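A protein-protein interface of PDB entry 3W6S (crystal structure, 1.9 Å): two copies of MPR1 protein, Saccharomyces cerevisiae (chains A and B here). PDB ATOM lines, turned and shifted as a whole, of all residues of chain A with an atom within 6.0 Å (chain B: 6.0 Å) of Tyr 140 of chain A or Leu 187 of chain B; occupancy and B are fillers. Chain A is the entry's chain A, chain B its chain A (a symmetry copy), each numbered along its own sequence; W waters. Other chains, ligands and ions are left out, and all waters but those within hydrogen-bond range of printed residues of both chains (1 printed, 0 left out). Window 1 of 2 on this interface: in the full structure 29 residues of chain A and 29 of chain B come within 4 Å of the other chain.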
ATOM      1  N   PRO A 138       9.489   0.992  29.130  1.00  0.00           N
ATOM      2  CA  PRO A 138       8.762   0.270  28.081  1.00  0.00           C
ATOM      3  C   PRO A 138       9.611   0.153  26.838  1.00  0.00           C
ATOM      4  O   PRO A 138      10.221   1.135  26.449  1.00  0.00           O
ATOM      5  CB  PRO A 138       7.578   1.181  27.789  1.00  0.00           C
ATOM      6  CG  PRO A 138       7.367   1.939  29.067  1.00  0.00           C
ATOM      7  CD  PRO A 138       8.756   2.182  29.587  1.00  0.00           C
ATOM      8  N   ASN A 139       9.655  -1.021  26.224  1.00  0.00           N
ATOM      9  CA  ASN A 139      10.476  -1.205  25.050  1.00  0.00           C
ATOM     10  C   ASN A 139       9.758  -0.684  23.816  1.00  0.00           C
ATOM     11  O   ASN A 139      10.389  -0.412  22.801  1.00  0.00           O
ATOM     12  CB  ASN A 139      10.826  -2.675  24.870  1.00  0.00           C
ATOM     13  CG  ASN A 139      11.959  -2.876  23.917  1.00  0.00           C
ATOM     14  OD1 ASN A 139      13.016  -2.274  24.064  1.00  0.00           O
ATOM     15  ND2 ASN A 139      11.749  -3.718  22.924  1.00  0.00           N
ATOM     16  N   TYR A 140       8.444  -0.517  23.923  1.00  0.00           N
ATOM     17  CA  TYR A 140       7.650  -0.036  22.807  1.00  0.00           C
ATOM     18  C   TYR A 140       6.617   0.999  23.205  1.00  0.00           C
ATOM     19  O   TYR A 140       6.382   1.241  24.388  1.00  0.00           O
ATOM     20  CB  TYR A 140       6.869  -1.176  22.181  1.00  0.00           C
ATOM     21  CG  TYR A 140       7.655  -2.415  21.894  1.00  0.00           C
ATOM     22  CD1 TYR A 140       8.508  -2.486  20.811  1.00  0.00           C
ATOM     23  CD2 TYR A 140       7.498  -3.536  22.679  1.00  0.00           C
ATOM     24  CE1 TYR A 140       9.202  -3.626  20.541  1.00  0.00           C
ATOM     25  CE2 TYR A 140       8.183  -4.675  22.422  1.00  0.00           C
ATOM     26  CZ  TYR A 140       9.033  -4.716  21.349  1.00  0.00           C
ATOM     27  OH  TYR A 140       9.730  -5.854  21.064  1.00  0.00           O
ATOM     28  N   ALA A 141       5.969   1.558  22.181  1.00  0.00           N
ATOM     29  CA  ALA A 141       4.825   2.451  22.335  1.00  0.00           C
ATOM     30  C   ALA A 141       3.648   1.720  22.996  1.00  0.00           C
ATOM     31  O   ALA A 141       3.623   0.496  23.024  1.00  0.00           O
ATOM     32  CB  ALA A 141       4.433   3.016  20.966  1.00  0.00           C
ATOM     33  N   PRO A 142       2.666   2.480  23.525  1.00  0.00           N
ATOM     34  CA  PRO A 142       1.600   2.088  24.462  1.00  0.00           C
ATOM     35  C   PRO A 142       0.933   0.731  24.279  1.00  0.00           C
ATOM     36  O   PRO A 142       0.748   0.041  25.285  1.00  0.00           O
ATOM     37  CB  PRO A 142       0.576   3.197  24.269  1.00  0.00           C
ATOM     38  CG  PRO A 142       1.431   4.389  24.100  1.00  0.00           C
ATOM     39  CD  PRO A 142       2.560   3.915  23.208  1.00  0.00           C
ATOM     40  N   CYS A 144       2.024  -1.874  23.217  1.00  0.00           N
ATOM     41  CA  CYS A 144       2.960  -2.943  23.520  1.00  0.00           C
ATOM     42  C   CYS A 144       3.825  -2.607  24.720  1.00  0.00           C
ATOM     43  O   CYS A 144       4.844  -3.235  24.931  1.00  0.00           O
ATOM     44  CB  CYS A 144       3.861  -3.224  22.309  1.00  0.00           C
ATOM     45  SG  CYS A 144       2.944  -3.619  20.791  1.00  0.00           S
ATOM     46  N   SER A 145       3.409  -1.620  25.504  1.00  0.00           N
ATOM     47  CA  SER A 145       4.254  -1.048  26.548  1.00  0.00           C
ATOM     48  C   SER A 145       4.356  -1.923  27.786  1.00  0.00           C
ATOM     49  O   SER A 145       5.048  -1.572  28.737  1.00  0.00           O
ATOM     50  CB  SER A 145       3.729   0.328  26.947  1.00  0.00           C
ATOM     51  OG  SER A 145       2.401   0.237  27.402  1.00  0.00           O
ATOM     52  N   ASN A 147       5.768  -4.654  27.577  1.00  0.00           N
ATOM     53  CA  ASN A 147       7.086  -5.221  27.389  1.00  0.00           C
ATOM     54  C   ASN A 147       8.095  -4.209  27.908  1.00  0.00           C
ATOM     55  O   ASN A 147       8.124  -3.072  27.436  1.00  0.00           O
ATOM     56  CB  ASN A 147       7.353  -5.505  25.901  1.00  0.00           C
ATOM     57  CG  ASN A 147       6.379  -6.510  25.313  1.00  0.00           C
ATOM     58  OD1 ASN A 147       6.582  -7.713  25.436  1.00  0.00           O
ATOM     59  ND2 ASN A 147       5.314  -6.028  24.677  1.00  0.00           N
ATOM     60  N   ILE A 184      12.167  -7.555  27.253  1.00  0.00           N
ATOM     61  CA  ILE A 184      12.866  -7.630  25.970  1.00  0.00           C
ATOM     62  C   ILE A 184      14.232  -6.963  26.055  1.00  0.00           C
ATOM     63  O   ILE A 184      14.335  -5.802  26.437  1.00  0.00           O
ATOM     64  CB  ILE A 184      12.096  -6.929  24.820  1.00  0.00           C
ATOM     65  CG1 ILE A 184      10.647  -7.407  24.751  1.00  0.00           C
ATOM     66  CG2 ILE A 184      12.782  -7.198  23.479  1.00  0.00           C
ATOM     67  CD1 ILE A 184      10.489  -8.800  24.126  1.00  0.00           C
ATOM     68  N   ASN A 186      16.838  -6.048  23.213  1.00  0.00           N
ATOM     69  CA  ASN A 186      16.873  -6.013  21.767  1.00  0.00           C
ATOM     70  C   ASN A 186      18.238  -6.356  21.205  1.00  0.00           C
ATOM     71  O   ASN A 186      18.336  -6.904  20.114  1.00  0.00           O
ATOM     72  CB  ASN A 186      16.492  -4.621  21.275  1.00  0.00           C
ATOM     73  CG  ASN A 186      15.187  -4.121  21.857  1.00  0.00           C
ATOM     74  OD1 ASN A 186      14.117  -4.562  21.469  1.00  0.00           O
ATOM     75  ND2 ASN A 186      15.274  -3.170  22.765  1.00  0.00           N
ATOM     76  N   THR B  88      -2.181  -2.411  13.738  1.00  0.00           N
ATOM     77  CA  THR B  88      -0.975  -2.508  12.926  1.00  0.00           C
ATOM     78  C   THR B  88       0.243  -1.909  13.615  1.00  0.00           C
ATOM     79  O   THR B  88       1.334  -2.474  13.576  1.00  0.00           O
ATOM     80  CB  THR B  88      -1.158  -1.769  11.591  1.00  0.00           C
ATOM     81  OG1 THR B  88      -2.108  -2.460  10.775  1.00  0.00           O
ATOM     82  CG2 THR B  88       0.167  -1.674  10.836  1.00  0.00           C
ATOM     83  N   PRO B  90       1.988   0.115  17.166  1.00  0.00           N
ATOM     84  CA  PRO B  90       1.941   0.117  18.635  1.00  0.00           C
ATOM     85  C   PRO B  90       1.406   1.408  19.249  1.00  0.00           C
ATOM     86  O   PRO B  90       1.053   1.415  20.426  1.00  0.00           O
ATOM     87  CB  PRO B  90       3.406  -0.078  19.030  1.00  0.00           C
ATOM     88  CG  PRO B  90       4.178   0.489  17.886  1.00  0.00           C
ATOM     89  CD  PRO B  90       3.371   0.149  16.664  1.00  0.00           C
ATOM     90  N   PHE B 185      12.423  -5.471  10.933  1.00  0.00           N
ATOM     91  CA  PHE B 185      11.127  -5.024  11.409  1.00  0.00           C
ATOM     92  C   PHE B 185      10.930  -5.605  12.796  1.00  0.00           C
ATOM     93  O   PHE B 185      10.904  -6.813  12.970  1.00  0.00           O
ATOM     94  CB  PHE B 185      10.009  -5.485  10.490  1.00  0.00           C
ATOM     95  CG  PHE B 185      10.234  -5.141   9.060  1.00  0.00           C
ATOM     96  CD1 PHE B 185      11.012  -4.066   8.712  1.00  0.00           C
ATOM     97  CD2 PHE B 185       9.698  -5.915   8.068  1.00  0.00           C
ATOM     98  CE1 PHE B 185      11.229  -3.759   7.400  1.00  0.00           C
ATOM     99  CE2 PHE B 185       9.918  -5.610   6.754  1.00  0.00           C
ATOM    100  CZ  PHE B 185      10.690  -4.527   6.418  1.00  0.00           C
ATOM    101  N   ASN B 186      10.807  -4.729  13.777  1.00  0.00           N
ATOM    102  CA  ASN B 186      10.782  -5.134  15.166  1.00  0.00           C
ATOM    103  C   ASN B 186       9.438  -5.693  15.589  1.00  0.00           C
ATOM    104  O   ASN B 186       9.372  -6.549  16.462  1.00  0.00           O
ATOM    105  CB  ASN B 186      11.102  -3.939  16.059  1.00  0.00           C
ATOM    106  CG  ASN B 186      12.378  -3.228  15.664  1.00  0.00           C
ATOM    107  OD1 ASN B 186      13.470  -3.716  15.908  1.00  0.00           O
ATOM    108  ND2 ASN B 186      12.242  -2.052  15.086  1.00  0.00           N
ATOM    109  N   LEU B 187       8.368  -5.195  14.981  1.00  0.00           N
ATOM    110  CA  LEU B 187       7.015  -5.625  15.319  1.00  0.00           C
ATOM    111  C   LEU B 187       6.151  -5.807  14.091  1.00  0.00           C
ATOM    112  O   LEU B 187       5.665  -4.835  13.524  1.00  0.00           O
ATOM    113  CB  LEU B 187       6.324  -4.584  16.180  1.00  0.00           C
ATOM    114  CG  LEU B 187       6.821  -4.428  17.603  1.00  0.00           C
ATOM    115  CD1 LEU B 187       6.108  -3.236  18.220  1.00  0.00           C
ATOM    116  CD2 LEU B 187       6.569  -5.710  18.392  1.00  0.00           C
ATOM    117  N   VAL B 188       5.945  -7.046  13.671  1.00  0.00           N
ATOM    118  CA  VAL B 188       4.901  -7.314  12.695  1.00  0.00           C
ATOM    119  C   VAL B 188       3.863  -8.292  13.273  1.00  0.00           C
ATOM    120  O   VAL B 188       4.138  -9.476  13.436  1.00  0.00           O
ATOM    121  CB  VAL B 188       5.474  -7.873  11.384  1.00  0.00           C
ATOM    122  CG1 VAL B 188       4.332  -8.292  10.455  1.00  0.00           C
ATOM    123  CG2 VAL B 188       6.379  -6.833  10.717  1.00  0.00           C
ATOM    124  N   PHE B 189       2.674  -7.790  13.575  1.00  0.00           N
ATOM    125  CA  PHE B 189       1.644  -8.597  14.200  1.00  0.00           C
ATOM    126  C   PHE B 189       1.166  -9.711  13.300  1.00  0.00           C
ATOM    127  O   PHE B 189       0.895  -9.507  12.127  1.00  0.00           O
ATOM    128  CB  PHE B 189       0.484  -7.712  14.602  1.00  0.00           C
ATOM    129  CG  PHE B 189       0.855  -6.727  15.652  1.00  0.00           C
ATOM    130  CD1 PHE B 189       1.185  -7.162  16.922  1.00  0.00           C
ATOM    131  CD2 PHE B 189       0.919  -5.382  15.376  1.00  0.00           C
ATOM    132  CE1 PHE B 189       1.556  -6.271  17.902  1.00  0.00           C
ATOM    133  CE2 PHE B 189       1.286  -4.487  16.357  1.00  0.00           C
ATOM    134  CZ  PHE B 189       1.608  -4.936  17.626  1.00  0.00           C
ATOM    135  N   VAL B 210       7.747 -12.339  19.439  1.00  0.00           N
ATOM    136  CA  VAL B 210       7.425 -11.818  20.750  1.00  0.00           C
ATOM    137  C   VAL B 210       6.000 -12.225  21.102  1.00  0.00           C
ATOM    138  O   VAL B 210       5.053 -11.840  20.434  1.00  0.00           O
ATOM    139  CB  VAL B 210       7.554 -10.304  20.764  1.00  0.00           C
ATOM    140  CG1 VAL B 210       7.226  -9.752  22.150  1.00  0.00           C
ATOM    141  CG2 VAL B 210       8.967  -9.903  20.341  1.00  0.00           C
ATOM    142  N   ALA B 213       2.682  -9.747  22.299  1.00  0.00           N
ATOM    143  CA  ALA B 213       3.350  -8.462  22.181  1.00  0.00           C
ATOM    144  C   ALA B 213       2.422  -7.270  22.296  1.00  0.00           C
ATOM    145  O   ALA B 213       2.780  -6.273  22.913  1.00  0.00           O
ATOM    146  CB  ALA B 213       4.082  -8.384  20.861  1.00  0.00           C
ATOM    147  N   ALA B 225       3.866 -10.999  17.915  1.00  0.00           N
ATOM    148  CA  ALA B 225       4.468 -10.190  16.870  1.00  0.00           C
ATOM    149  C   ALA B 225       5.706 -10.881  16.330  1.00  0.00           C
ATOM    150  O   ALA B 225       6.468 -11.479  17.077  1.00  0.00           O
ATOM    151  CB  ALA B 225       4.820  -8.801  17.397  1.00  0.00           C
ATOM    152  N   ILE B 226       5.887 -10.807  15.020  1.00  0.00           N
ATOM    153  CA  ILE B 226       7.051 -11.376  14.377  1.00  0.00           C
ATOM    154  C   ILE B 226       8.137 -10.323  14.242  1.00  0.00           C
ATOM    155  O   ILE B 226       7.863  -9.137  13.993  1.00  0.00           O
ATOM    156  CB  ILE B 226       6.696 -11.884  12.982  1.00  0.00           C
ATOM    157  CG1 ILE B 226       5.685 -13.012  13.104  1.00  0.00           C
ATOM    158  CG2 ILE B 226       7.932 -12.385  12.240  1.00  0.00           C
ATOM    159  CD1 ILE B 226       4.749 -13.097  11.932  1.00  0.00           C
ATOM    160  N   ILE B 227       9.375 -10.769  14.377  1.00  0.00           N
ATOM    161  CA  ILE B 227      10.513  -9.938  14.063  1.00  0.00           C
ATOM    162  C   ILE B 227      11.129 -10.419  12.753  1.00  0.00           C
ATOM    163  O   ILE B 227      11.586 -11.551  12.679  1.00  0.00           O
ATOM    164  CB  ILE B 227      11.520 -10.027  15.194  1.00  0.00           C
ATOM    165  CG1 ILE B 227      10.806  -9.699  16.505  1.00  0.00           C
ATOM    166  CG2 ILE B 227      12.699  -9.093  14.939  1.00  0.00           C
ATOM    167  CD1 ILE B 227      11.715  -9.682  17.697  1.00  0.00           C
HETATM  168  O   HOH W   1      11.023  -5.863  18.548  1.00  0.00           O
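O of Ala 213 of chain B sits close to SG of Cys 144 of chain A (3.4 Å). ND2 of Asn 147 of chain A lies within hydrogen-bond range of O of Ala 213 of chain B, 3.1 Å away.
The side-chain amide nitrogen (ND2) of Asn 139 of chain A lies close to the side-chain hydroxyl (OH) of Tyr 140 of chain A (3.5 Å). The backbone carbonyl oxygen (O) of Pro 142 of chain A is in hydrogen-bond range of the side-chain hydroxyl (OG) of Ser 145 of chain A. The backbone carbonyl oxygen (O) of Asn 147 of chain A is in hydrogen-bond range of the backbone NH (N) of Asn 139 of chain A (2.8 Å). N of Val 210 of chain B sits at hydrogen-bond distance from O of Ala 225 of chain B. ND2 of Asn 147 of chain A sits at hydrogen-bond distance from O of Cys 144 of chain A (2.8 Å).
Leu 187 of chain B touches Tyr 140 of chain A (CD1 to CD1, 3.6 Å). Ala 141 of chain A touches Pro 90 of chain B (C to O, 3.7 Å). Pro 90 of chain B touches Pro 142 of chain A (O to N, 3.7 Å). Cys 144 of chain A touches Pro 90 of chain B (SG to CB, 3.98 Å). Phe 189 of chain B touches Cys 144 of chain A (CZ to SG, 3.7 Å). OD1 of Asn 147 of chain A touches CG1 of Val 210 of chain B (3.9 Å). Ile 184 of chain A touches Val 210 of chain B (CD1 to CG1, 3.9 Å).
Tyr 140 of chain A touches one residue of chain B. Of chain A, only Tyr 140 comes within 4 Å of Leu 187 of chain B. Of the printed residues of chain A, Phe 189 of chain B touches Cys 144 (3.7 Å). Printed residues of chain B within 4 Å of Asn 147 of chain A: Val 210 and Ala 213. Printed residues of chain B within 4 Å of Ile 184 of chain A: Val 210 (3.9 Å). Of the printed residues of chain A, Ala 213 of chain B touches Cys 144 (3.3 Å) and Asn 147 (3.1 Å). Of the printed residues of chain B, Cys 144 of chain A touches Pro 90, Phe 189 and Ala 213. The nearest printed residue of chain A that does not touch Ala 213 of chain B is Ser 145 of chain A (5.4 Å).
Of the 12 printed residues of chain B, 5 touch a printed residue of chain A. Hydrophobic or aromatic side chains of chain B within 4 Å of the printed part of chain A: Pro 90, Leu 187, Phe 189 and Val 210. Of the 10 printed residues of chain A, 6 touch a printed residue of chain B. Hydrophobic or aromatic side chains of chain A that line the printed part of chain B: Tyr 140, Ala 141 and Ile 184. Among the printed residues, no Asp or Glu carboxylate lies within 4 Å of a Lys or Arg side-chain nitrogen of the other chain.
Position printed for both chains: 186. Of the 9 pairs that touch across the chains among the printed residues, none has its exchanged pair printed and touching as well.
Water W1 bridges O of Asn 186 of chain B and OH of Tyr 140 of chain A.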
